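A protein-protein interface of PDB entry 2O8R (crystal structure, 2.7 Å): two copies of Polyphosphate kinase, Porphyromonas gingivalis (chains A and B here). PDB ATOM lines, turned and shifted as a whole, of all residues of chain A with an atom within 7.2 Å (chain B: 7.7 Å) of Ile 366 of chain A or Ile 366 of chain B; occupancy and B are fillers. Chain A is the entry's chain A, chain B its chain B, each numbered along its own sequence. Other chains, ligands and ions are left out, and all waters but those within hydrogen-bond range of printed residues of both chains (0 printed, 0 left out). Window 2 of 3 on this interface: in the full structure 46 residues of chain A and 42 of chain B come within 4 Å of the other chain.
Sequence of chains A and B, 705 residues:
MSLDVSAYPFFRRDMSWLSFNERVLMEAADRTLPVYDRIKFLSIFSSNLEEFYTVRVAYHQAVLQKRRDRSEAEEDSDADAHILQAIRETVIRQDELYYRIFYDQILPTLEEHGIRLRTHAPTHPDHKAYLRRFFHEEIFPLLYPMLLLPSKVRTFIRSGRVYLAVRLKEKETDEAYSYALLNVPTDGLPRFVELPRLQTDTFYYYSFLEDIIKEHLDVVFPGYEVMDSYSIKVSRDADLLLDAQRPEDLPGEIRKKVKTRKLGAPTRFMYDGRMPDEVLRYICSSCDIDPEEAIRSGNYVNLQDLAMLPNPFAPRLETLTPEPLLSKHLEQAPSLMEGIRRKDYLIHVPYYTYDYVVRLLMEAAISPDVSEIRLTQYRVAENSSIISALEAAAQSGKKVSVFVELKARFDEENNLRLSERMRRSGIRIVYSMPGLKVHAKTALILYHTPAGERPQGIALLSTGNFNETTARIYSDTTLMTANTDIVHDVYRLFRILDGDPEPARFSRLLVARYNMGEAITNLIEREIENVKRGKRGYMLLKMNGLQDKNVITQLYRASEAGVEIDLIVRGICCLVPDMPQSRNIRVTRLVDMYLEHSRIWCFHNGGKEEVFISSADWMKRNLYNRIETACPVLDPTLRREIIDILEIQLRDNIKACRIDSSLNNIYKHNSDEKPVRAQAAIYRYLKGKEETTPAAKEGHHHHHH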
ATOM      1  N   ARG A 359      34.022  13.082  -0.483  1.00  0.00           N
ATOM      2  CA  ARG A 359      33.981  12.730  -1.905  1.00  0.00           C
ATOM      3  C   ARG A 359      32.842  11.753  -2.226  1.00  0.00           C
ATOM      4  O   ARG A 359      32.074  11.951  -3.177  1.00  0.00           O
ATOM      5  CB  ARG A 359      35.284  12.050  -2.283  1.00  0.00           C
ATOM      6  CG  ARG A 359      35.963  12.641  -3.459  1.00  0.00           C
ATOM      7  CD  ARG A 359      37.301  13.160  -3.029  1.00  0.00           C
ATOM      8  NE  ARG A 359      38.449  12.301  -3.355  1.00  0.00           N
ATOM      9  CZ  ARG A 359      38.538  11.433  -4.362  1.00  0.00           C
ATOM     10  NH1 ARG A 359      39.657  10.750  -4.528  1.00  0.00           N
ATOM     11  NH2 ARG A 359      37.545  11.246  -5.218  1.00  0.00           N
ATOM     12  N   LEU A 360      32.760  10.692  -1.425  1.00  0.00           N
ATOM     13  CA  LEU A 360      31.712   9.704  -1.550  1.00  0.00           C
ATOM     14  C   LEU A 360      30.364  10.360  -1.320  1.00  0.00           C
ATOM     15  O   LEU A 360      29.446  10.217  -2.126  1.00  0.00           O
ATOM     16  CB  LEU A 360      31.917   8.568  -0.549  1.00  0.00           C
ATOM     17  CG  LEU A 360      31.050   7.368  -0.905  1.00  0.00           C
ATOM     18  CD1 LEU A 360      31.565   6.765  -2.197  1.00  0.00           C
ATOM     19  CD2 LEU A 360      31.070   6.344   0.197  1.00  0.00           C
ATOM     20  N   LEU A 361      30.262  11.102  -0.227  1.00  0.00           N
ATOM     21  CA  LEU A 361      29.048  11.852   0.060  1.00  0.00           C
ATOM     22  C   LEU A 361      28.650  12.750  -1.101  1.00  0.00           C
ATOM     23  O   LEU A 361      27.471  12.841  -1.433  1.00  0.00           O
ATOM     24  CB  LEU A 361      29.190  12.663   1.345  1.00  0.00           C
ATOM     25  CG  LEU A 361      29.057  11.821   2.616  1.00  0.00           C
ATOM     26  CD1 LEU A 361      29.356  12.666   3.835  1.00  0.00           C
ATOM     27  CD2 LEU A 361      27.676  11.194   2.715  1.00  0.00           C
ATOM     28  N   MET A 362      29.631  13.381  -1.738  1.00  0.00           N
ATOM     29  CA  MET A 362      29.359  14.260  -2.874  1.00  0.00           C
ATOM     30  C   MET A 362      28.906  13.494  -4.109  1.00  0.00           C
ATOM     31  O   MET A 362      28.017  13.952  -4.824  1.00  0.00           O
ATOM     32  CB  MET A 362      30.571  15.114  -3.209  1.00  0.00           C
ATOM     33  CG  MET A 362      30.820  16.234  -2.232  1.00  0.00           C
ATOM     34  SD  MET A 362      32.399  17.261  -2.736  1.00  0.00           S
ATOM     35  CE  MET A 362      33.825  16.192  -1.988  1.00  0.00           C
ATOM     36  N   GLU A 363      29.512  12.335  -4.358  1.00  0.00           N
ATOM     37  CA  GLU A 363      29.038  11.469  -5.438  1.00  0.00           C
ATOM     38  C   GLU A 363      27.581  11.177  -5.202  1.00  0.00           C
ATOM     39  O   GLU A 363      26.749  11.469  -6.058  1.00  0.00           O
ATOM     40  CB  GLU A 363      29.844  10.162  -5.534  1.00  0.00           C
ATOM     41  CG  GLU A 363      31.090  10.331  -6.376  1.00  0.00           C
ATOM     42  CD  GLU A 363      31.794   9.039  -6.740  1.00  0.00           C
ATOM     43  OE1 GLU A 363      31.247   7.936  -6.504  1.00  0.00           O
ATOM     44  OE2 GLU A 363      32.922   9.140  -7.272  1.00  0.00           O
ATOM     45  N   ALA A 364      27.285  10.648  -4.014  1.00  0.00           N
ATOM     46  CA  ALA A 364      25.926  10.288  -3.603  1.00  0.00           C
ATOM     47  C   ALA A 364      24.939  11.441  -3.721  1.00  0.00           C
ATOM     48  O   ALA A 364      23.752  11.218  -3.963  1.00  0.00           O
ATOM     49  CB  ALA A 364      25.929   9.752  -2.178  1.00  0.00           C
ATOM     50  N   ALA A 365      25.432  12.664  -3.551  1.00  0.00           N
ATOM     51  CA  ALA A 365      24.575  13.839  -3.570  1.00  0.00           C
ATOM     52  C   ALA A 365      23.887  13.988  -4.922  1.00  0.00           C
ATOM     53  O   ALA A 365      22.668  14.130  -4.990  1.00  0.00           O
ATOM     54  CB  ALA A 365      25.367  15.087  -3.231  1.00  0.00           C
ATOM     55  N   ILE A 366      24.667  13.911  -5.993  1.00  0.00           N
ATOM     56  CA  ILE A 366      24.134  14.128  -7.336  1.00  0.00           C
ATOM     57  C   ILE A 366      23.798  12.839  -8.100  1.00  0.00           C
ATOM     58  O   ILE A 366      23.536  12.882  -9.303  1.00  0.00           O
ATOM     59  CB  ILE A 366      25.066  15.026  -8.183  1.00  0.00           C
ATOM     60  CG1 ILE A 366      26.460  14.417  -8.291  1.00  0.00           C
ATOM     61  CG2 ILE A 366      25.129  16.434  -7.596  1.00  0.00           C
ATOM     62  CD1 ILE A 366      27.238  14.907  -9.500  1.00  0.00           C
ATOM     63  N   SER A 367      23.793  11.701  -7.407  1.00  0.00           N
ATOM     64  CA  SER A 367      23.418  10.444  -8.045  1.00  0.00           C
ATOM     65  C   SER A 367      21.926  10.149  -7.963  1.00  0.00           C
ATOM     66  O   SER A 367      21.366  10.083  -6.872  1.00  0.00           O
ATOM     67  CB  SER A 367      24.178   9.264  -7.450  1.00  0.00           C
ATOM     68  OG  SER A 367      23.498   8.056  -7.765  1.00  0.00           O
ATOM     69  N   PRO A 368      21.287   9.940  -9.127  1.00  0.00           N
ATOM     70  CA  PRO A 368      19.901   9.480  -9.261  1.00  0.00           C
ATOM     71  C   PRO A 368      19.569   8.201  -8.482  1.00  0.00           C
ATOM     72  O   PRO A 368      18.421   8.019  -8.069  1.00  0.00           O
ATOM     73  CB  PRO A 368      19.768   9.199 -10.764  1.00  0.00           C
ATOM     74  CG  PRO A 368      21.173   9.197 -11.301  1.00  0.00           C
ATOM     75  CD  PRO A 368      21.903  10.166 -10.443  1.00  0.00           C
ATOM     76  N   ASP A 369      20.558   7.330  -8.281  1.00  0.00           N
ATOM     77  CA  ASP A 369      20.314   6.026  -7.655  1.00  0.00           C
ATOM     78  C   ASP A 369      20.106   6.066  -6.141  1.00  0.00           C
ATOM     79  O   ASP A 369      19.564   5.124  -5.570  1.00  0.00           O
ATOM     80  CB  ASP A 369      21.447   5.053  -7.982  1.00  0.00           C
ATOM     81  CG  ASP A 369      21.678   4.893  -9.483  1.00  0.00           C
ATOM     82  OD1 ASP A 369      20.821   5.328 -10.286  1.00  0.00           O
ATOM     83  OD2 ASP A 369      22.725   4.316  -9.858  1.00  0.00           O
ATOM     84  N   VAL A 370      20.533   7.149  -5.496  1.00  0.00           N
ATOM     85  CA  VAL A 370      20.526   7.224  -4.035  1.00  0.00           C
ATOM     86  C   VAL A 370      19.182   7.721  -3.507  1.00  0.00           C
ATOM     87  O   VAL A 370      18.701   8.782  -3.901  1.00  0.00           O
ATOM     88  CB  VAL A 370      21.657   8.151  -3.490  1.00  0.00           C
ATOM     89  CG1 VAL A 370      21.740   8.079  -1.966  1.00  0.00           C
ATOM     90  CG2 VAL A 370      22.994   7.803  -4.101  1.00  0.00           C
ATOM     91  N   SER A 388      28.166  20.295   4.180  1.00  0.00           N
ATOM     92  CA  SER A 388      27.907  20.857   2.875  1.00  0.00           C
ATOM     93  C   SER A 388      27.457  19.804   1.873  1.00  0.00           C
ATOM     94  O   SER A 388      26.455  19.999   1.173  1.00  0.00           O
ATOM     95  CB  SER A 388      29.137  21.587   2.376  1.00  0.00           C
ATOM     96  OG  SER A 388      29.176  22.895   2.925  1.00  0.00           O
ATOM     97  N   ALA A 389      28.178  18.687   1.820  1.00  0.00           N
ATOM     98  CA  ALA A 389      27.796  17.592   0.932  1.00  0.00           C
ATOM     99  C   ALA A 389      26.401  17.102   1.291  1.00  0.00           C
ATOM    100  O   ALA A 389      25.596  16.829   0.411  1.00  0.00           O
ATOM    101  CB  ALA A 389      28.803  16.455   0.992  1.00  0.00           C
ATOM    102  N   ALA A 392      23.664  19.684   0.135  1.00  0.00           N
ATOM    103  CA  ALA A 392      23.462  19.435  -1.293  1.00  0.00           C
ATOM    104  C   ALA A 392      22.510  18.264  -1.547  1.00  0.00           C
ATOM    105  O   ALA A 392      21.608  18.352  -2.386  1.00  0.00           O
ATOM    106  CB  ALA A 392      24.810  19.177  -1.986  1.00  0.00           C
ATOM    107  N   ALA A 393      22.714  17.174  -0.812  1.00  0.00           N
ATOM    108  CA  ALA A 393      21.934  15.966  -0.999  1.00  0.00           C
ATOM    109  C   ALA A 393      20.487  16.186  -0.599  1.00  0.00           C
ATOM    110  O   ALA A 393      19.575  15.758  -1.306  1.00  0.00           O
ATOM    111  CB  ALA A 393      22.533  14.829  -0.211  1.00  0.00           C
ATOM    112  N   SER A 396      18.825  18.113  -3.042  1.00  0.00           N
ATOM    113  CA  SER A 396      18.566  17.255  -4.194  1.00  0.00           C
ATOM    114  C   SER A 396      17.457  16.261  -3.918  1.00  0.00           C
ATOM    115  O   SER A 396      17.314  15.282  -4.653  1.00  0.00           O
ATOM    116  CB  SER A 396      19.820  16.484  -4.592  1.00  0.00           C
ATOM    117  OG  SER A 396      20.319  16.940  -5.833  1.00  0.00           O
ATOM    118  N   LYS A 398      16.935  14.022  -1.569  1.00  0.00           N
ATOM    119  CA  LYS A 398      17.241  12.741  -0.933  1.00  0.00           C
ATOM    120  C   LYS A 398      17.039  12.831   0.568  1.00  0.00           C
ATOM    121  O   LYS A 398      17.351  13.855   1.176  1.00  0.00           O
ATOM    122  CB  LYS A 398      18.684  12.327  -1.234  1.00  0.00           C
ATOM    123  CG  LYS A 398      19.182  12.790  -2.589  1.00  0.00           C
ATOM    124  CD  LYS A 398      20.337  11.960  -3.081  1.00  0.00           C
ATOM    125  CE  LYS A 398      20.252  11.785  -4.585  1.00  0.00           C
ATOM    126  NZ  LYS A 398      20.126  13.081  -5.305  1.00  0.00           N
ATOM    127  N   MET B 337      24.890  27.294 -12.487  1.00  0.00           N
ATOM    128  CA  MET B 337      26.022  27.418 -13.390  1.00  0.00           C
ATOM    129  C   MET B 337      25.546  27.531 -14.828  1.00  0.00           C
ATOM    130  O   MET B 337      26.116  28.282 -15.616  1.00  0.00           O
ATOM    131  CB  MET B 337      26.960  26.229 -13.240  1.00  0.00           C
ATOM    132  CG  MET B 337      27.565  26.098 -11.867  1.00  0.00           C
ATOM    133  SD  MET B 337      28.977  24.782 -11.811  1.00  0.00           S
ATOM    134  CE  MET B 337      30.353  25.866 -12.633  1.00  0.00           C
ATOM    135  N   LEU B 360      26.300  28.512  -5.570  1.00  0.00           N
ATOM    136  CA  LEU B 360      27.026  28.424  -6.827  1.00  0.00           C
ATOM    137  C   LEU B 360      28.341  27.741  -6.582  1.00  0.00           C
ATOM    138  O   LEU B 360      28.781  26.913  -7.386  1.00  0.00           O
ATOM    139  CB  LEU B 360      27.266  29.794  -7.467  1.00  0.00           C
ATOM    140  CG  LEU B 360      28.229  29.691  -8.659  1.00  0.00           C
ATOM    141  CD1 LEU B 360      27.588  28.994  -9.853  1.00  0.00           C
ATOM    142  CD2 LEU B 360      28.779  31.023  -9.062  1.00  0.00           C
ATOM    143  N   LEU B 361      28.971  28.087  -5.462  1.00  0.00           N
ATOM    144  CA  LEU B 361      30.255  27.490  -5.104  1.00  0.00           C
ATOM    145  C   LEU B 361      30.125  25.988  -4.904  1.00  0.00           C
ATOM    146  O   LEU B 361      30.952  25.227  -5.400  1.00  0.00           O
ATOM    147  CB  LEU B 361      30.872  28.181  -3.890  1.00  0.00           C
ATOM    148  CG  LEU B 361      31.556  29.527  -4.187  1.00  0.00           C
ATOM    149  CD1 LEU B 361      31.993  30.207  -2.881  1.00  0.00           C
ATOM    150  CD2 LEU B 361      32.745  29.361  -5.160  1.00  0.00           C
ATOM    151  N   MET B 362      29.057  25.560  -4.237  1.00  0.00           N
ATOM    152  CA  MET B 362      28.815  24.129  -4.072  1.00  0.00           C
ATOM    153  C   MET B 362      28.623  23.390  -5.383  1.00  0.00           C
ATOM    154  O   MET B 362      29.179  22.309  -5.560  1.00  0.00           O
ATOM    155  CB  MET B 362      27.628  23.832  -3.163  1.00  0.00           C
ATOM    156  CG  MET B 362      27.746  22.423  -2.574  1.00  0.00           C
ATOM    157  SD  MET B 362      29.369  22.279  -1.471  1.00  0.00           S
ATOM    158  CE  MET B 362      28.859  23.728  -0.256  1.00  0.00           C
ATOM    159  N   GLU B 363      27.826  23.971  -6.283  1.00  0.00           N
ATOM    160  CA  GLU B 363      27.630  23.416  -7.620  1.00  0.00           C
ATOM    161  C   GLU B 363      28.981  23.222  -8.266  1.00  0.00           C
ATOM    162  O   GLU B 363      29.224  22.195  -8.900  1.00  0.00           O
ATOM    163  CB  GLU B 363      26.801  24.345  -8.492  1.00  0.00           C
ATOM    164  CG  GLU B 363      25.315  24.280  -8.248  1.00  0.00           C
ATOM    165  CD  GLU B 363      24.519  24.853  -9.403  1.00  0.00           C
ATOM    166  OE1 GLU B 363      25.123  25.459 -10.303  1.00  0.00           O
ATOM    167  OE2 GLU B 363      23.286  24.699  -9.411  1.00  0.00           O
ATOM    168  N   ALA B 364      29.860  24.209  -8.066  1.00  0.00           N
ATOM    169  CA  ALA B 364      31.216  24.158  -8.581  1.00  0.00           C
ATOM    170  C   ALA B 364      32.052  23.062  -7.915  1.00  0.00           C
ATOM    171  O   ALA B 364      32.900  22.456  -8.559  1.00  0.00           O
ATOM    172  CB  ALA B 364      31.884  25.509  -8.430  1.00  0.00           C
ATOM    173  N   ALA B 365      31.794  22.810  -6.634  1.00  0.00           N
ATOM    174  CA  ALA B 365      32.523  21.794  -5.874  1.00  0.00           C
ATOM    175  C   ALA B 365      32.189  20.365  -6.324  1.00  0.00           C
ATOM    176  O   ALA B 365      33.087  19.529  -6.457  1.00  0.00           O
ATOM    177  CB  ALA B 365      32.271  21.971  -4.385  1.00  0.00           C
ATOM    178  N   ILE B 366      30.909  20.087  -6.573  1.00  0.00           N
ATOM    179  CA  ILE B 366      30.501  18.784  -7.111  1.00  0.00           C
ATOM    180  C   ILE B 366      30.718  18.604  -8.623  1.00  0.00           C
ATOM    181  O   ILE B 366      30.821  17.473  -9.101  1.00  0.00           O
ATOM    182  CB  ILE B 366      29.039  18.445  -6.778  1.00  0.00           C
ATOM    183  CG1 ILE B 366      28.654  18.984  -5.406  1.00  0.00           C
ATOM    184  CG2 ILE B 366      28.843  16.945  -6.754  1.00  0.00           C
ATOM    185  CD1 ILE B 366      27.224  18.664  -5.025  1.00  0.00           C
ATOM    186  N   SER B 367      30.796  19.696  -9.380  1.00  0.00           N
ATOM    187  CA  SER B 367      30.898  19.585 -10.845  1.00  0.00           C
ATOM    188  C   SER B 367      32.221  19.000 -11.313  1.00  0.00           C
ATOM    189  O   SER B 367      33.284  19.472 -10.911  1.00  0.00           O
ATOM    190  CB  SER B 367      30.687  20.933 -11.535  1.00  0.00           C
ATOM    191  OG  SER B 367      31.425  20.990 -12.749  1.00  0.00           O
ATOM    192  N   PRO B 368      32.153  17.976 -12.176  1.00  0.00           N
ATOM    193  CA  PRO B 368      33.341  17.384 -12.798  1.00  0.00           C
ATOM    194  C   PRO B 368      34.060  18.341 -13.752  1.00  0.00           C
ATOM    195  O   PRO B 368      35.276  18.219 -13.937  1.00  0.00           O
ATOM    196  CB  PRO B 368      32.780  16.178 -13.561  1.00  0.00           C
ATOM    197  CG  PRO B 368      31.340  16.476 -13.763  1.00  0.00           C
ATOM    198  CD  PRO B 368      30.911  17.296 -12.583  1.00  0.00           C
ATOM    199  N   ASP B 369      33.317  19.287 -14.327  1.00  0.00           N
ATOM    200  CA  ASP B 369      33.859  20.265 -15.278  1.00  0.00           C
ATOM    201  C   ASP B 369      34.780  21.320 -14.656  1.00  0.00           C
ATOM    202  O   ASP B 369      35.712  21.805 -15.310  1.00  0.00           O
ATOM    203  CB  ASP B 369      32.726  20.988 -16.005  1.00  0.00           C
ATOM    204  CG  ASP B 369      31.863  20.059 -16.832  1.00  0.00           C
ATOM    205  OD1 ASP B 369      31.416  19.021 -16.297  1.00  0.00           O
ATOM    206  OD2 ASP B 369      31.618  20.386 -18.015  1.00  0.00           O
ATOM    207  N   VAL B 370      34.506  21.694 -13.409  1.00  0.00           N
ATOM    208  CA  VAL B 370      35.262  22.767 -12.751  1.00  0.00           C
ATOM    209  C   VAL B 370      36.697  22.330 -12.462  1.00  0.00           C
ATOM    210  O   VAL B 370      36.931  21.305 -11.824  1.00  0.00           O
ATOM    211  CB  VAL B 370      34.571  23.245 -11.449  1.00  0.00           C
ATOM    212  CG1 VAL B 370      35.402  24.295 -10.747  1.00  0.00           C
ATOM    213  CG2 VAL B 370      33.199  23.776 -11.756  1.00  0.00           C
ATOM    214  N   ILE B 373      39.030  27.040  -8.403  1.00  0.00           N
ATOM    215  CA  ILE B 373      38.252  28.057  -7.716  1.00  0.00           C
ATOM    216  C   ILE B 373      39.175  29.032  -6.994  1.00  0.00           C
ATOM    217  O   ILE B 373      39.979  28.629  -6.153  1.00  0.00           O
ATOM    218  CB  ILE B 373      37.301  27.451  -6.683  1.00  0.00           C
ATOM    219  CG1 ILE B 373      36.279  26.528  -7.366  1.00  0.00           C
ATOM    220  CG2 ILE B 373      36.578  28.565  -5.924  1.00  0.00           C
ATOM    221  CD1 ILE B 373      35.112  26.110  -6.483  1.00  0.00           C
ATOM    222  N   ALA B 389      32.604  24.964   1.501  1.00  0.00           N
ATOM    223  CA  ALA B 389      32.418  24.713   0.065  1.00  0.00           C
ATOM    224  C   ALA B 389      33.754  24.582  -0.650  1.00  0.00           C
ATOM    225  O   ALA B 389      33.970  23.646  -1.423  1.00  0.00           O
ATOM    226  CB  ALA B 389      31.590  25.829  -0.571  1.00  0.00           C
ATOM    227  N   ALA B 392      35.353  21.459   0.281  1.00  0.00           N
ATOM    228  CA  ALA B 392      34.744  20.394  -0.508  1.00  0.00           C
ATOM    229  C   ALA B 392      35.287  20.375  -1.928  1.00  0.00           C
ATOM    230  O   ALA B 392      35.518  19.306  -2.490  1.00  0.00           O
ATOM    231  CB  ALA B 392      33.238  20.522  -0.524  1.00  0.00           C
ATOM    232  N   ALA B 393      35.499  21.554  -2.500  1.00  0.00           N
ATOM    233  CA  ALA B 393      36.036  21.637  -3.842  1.00  0.00           C
ATOM    234  C   ALA B 393      37.462  21.088  -3.883  1.00  0.00           C
ATOM    235  O   ALA B 393      37.792  20.250  -4.730  1.00  0.00           O
ATOM    236  CB  ALA B 393      35.982  23.063  -4.357  1.00  0.00           C
ATOM    237  N   SER B 396      37.552  17.361  -3.524  1.00  0.00           N
ATOM    238  CA  SER B 396      37.211  16.772  -4.831  1.00  0.00           C
ATOM    239  C   SER B 396      38.373  16.830  -5.815  1.00  0.00           C
ATOM    240  O   SER B 396      38.221  16.431  -6.968  1.00  0.00           O
ATOM    241  CB  SER B 396      36.022  17.486  -5.472  1.00  0.00           C
ATOM    242  OG  SER B 396      34.815  16.812  -5.184  1.00  0.00           O
ATOM    243  N   LYS B 398      40.132  19.697  -6.724  1.00  0.00           N
ATOM    244  CA  LYS B 398      40.221  20.917  -7.511  1.00  0.00           C
ATOM    245  C   LYS B 398      41.242  21.867  -6.917  1.00  0.00           C
ATOM    246  O   LYS B 398      41.448  21.882  -5.700  1.00  0.00           O
ATOM    247  CB  LYS B 398      38.849  21.584  -7.603  1.00  0.00           C
ATOM    248  CG  LYS B 398      37.759  20.607  -7.985  1.00  0.00           C
ATOM    249  CD  LYS B 398      36.522  21.285  -8.506  1.00  0.00           C
ATOM    250  CE  LYS B 398      35.384  20.280  -8.641  1.00  0.00           C
ATOM    251  NZ  LYS B 398      35.688  19.157  -9.576  1.00  0.00           N
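Of chain B, only Ile 366 (3.8 Å) comes within 4 Å of Ile 366 of chain A. Printed residues of chain A within 4 Å of Ile 366 of chain B: Met 362 (3.7 Å), Ile 366 (3.8 Å) and Ala 392 (3.9 Å). Printed residues of chain B within 4 Å of Met 362 of chain A: Ile 366, Ala 392 and Ser 396. Of the printed residues of chain A, Ser 396 of chain B touches Met 362. Printed residues of chain A within 4 Å of Ala 392 of chain B: Met 362. Ala 364 of chain B touches none of the printed residues of chain A. Met 337 of chain B touches none of the printed residues of chain A. The nearest residue of chain A that does not touch Ile 366 of chain B is Ala 365 of chain A (4.4 Å). The nearest printed residue of chain A that does not touch Ser 396 of chain B is Arg 359 of chain A (4.04 Å).
SD of Met 362 of chain A sits close to OG of Ser 396 of chain B (3.5 Å). O of Ala 392 of chain B sits close to SD of Met 362 of chain A (3.7 Å).
The side-chain hydroxyl (OG) of Ser 396 of chain B sits at hydrogen-bond distance from the backbone carbonyl oxygen (O) of Ala 365 of chain B.
Among the printed residues, pairs that only touch across the chains: Ser 388 of chain A with Met 362 of chain B, Met 362 of chain A with Ile 366 of chain B, Ile 366 of chain A with Ile 366 of chain B and Ala 392 of chain A with Ile 366 of chain B.
Of the 18 printed residues of chain A, 4 touch a printed residue of chain B. Hydrophobic or aromatic side chains of chain A that line the printed part of chain B: Met 362, Ile 366 and Ala 392. Along chain A the printed residues that touch a printed residue of chain B span positions 362 to 392. Printed residues of chain B that touch a printed residue of chain A: Met 362, Ile 366, Ala 392 and Ser 396. Hydrophobic or aromatic side chains of chain B within 4 Å of the printed part of chain A: Met 362 and Ile 366. Along chain B the printed residues that touch a printed residue of chain A span positions 362 to 396. Among the printed residues, 6 pairs touch across the chains.
Met 362 of chain A touches Ala 392 of chain B, but with the chains exchanged Ala 392 of chain A does not touch Met 362 of chain B (4.4 Å). Met 362 of chain A touches Ser 396 of chain B, but with the chains exchanged Ser 396 of chain A does not touch Met 362 of chain B (9.8 Å). Ile 366 of chain A touches its own counterpart, Ile 366 of chain B. Ala 392 of chain A touches Ile 366 of chain B, but with the chains exchanged Ile 366 of chain A does not touch Ala 392 of chain B (11.5 Å). Positions printed for both chains: 360, 361, 362, 363, 364, 365, 366, 367, 368, 369, 370, 389, 392, 393, 396 and 398.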
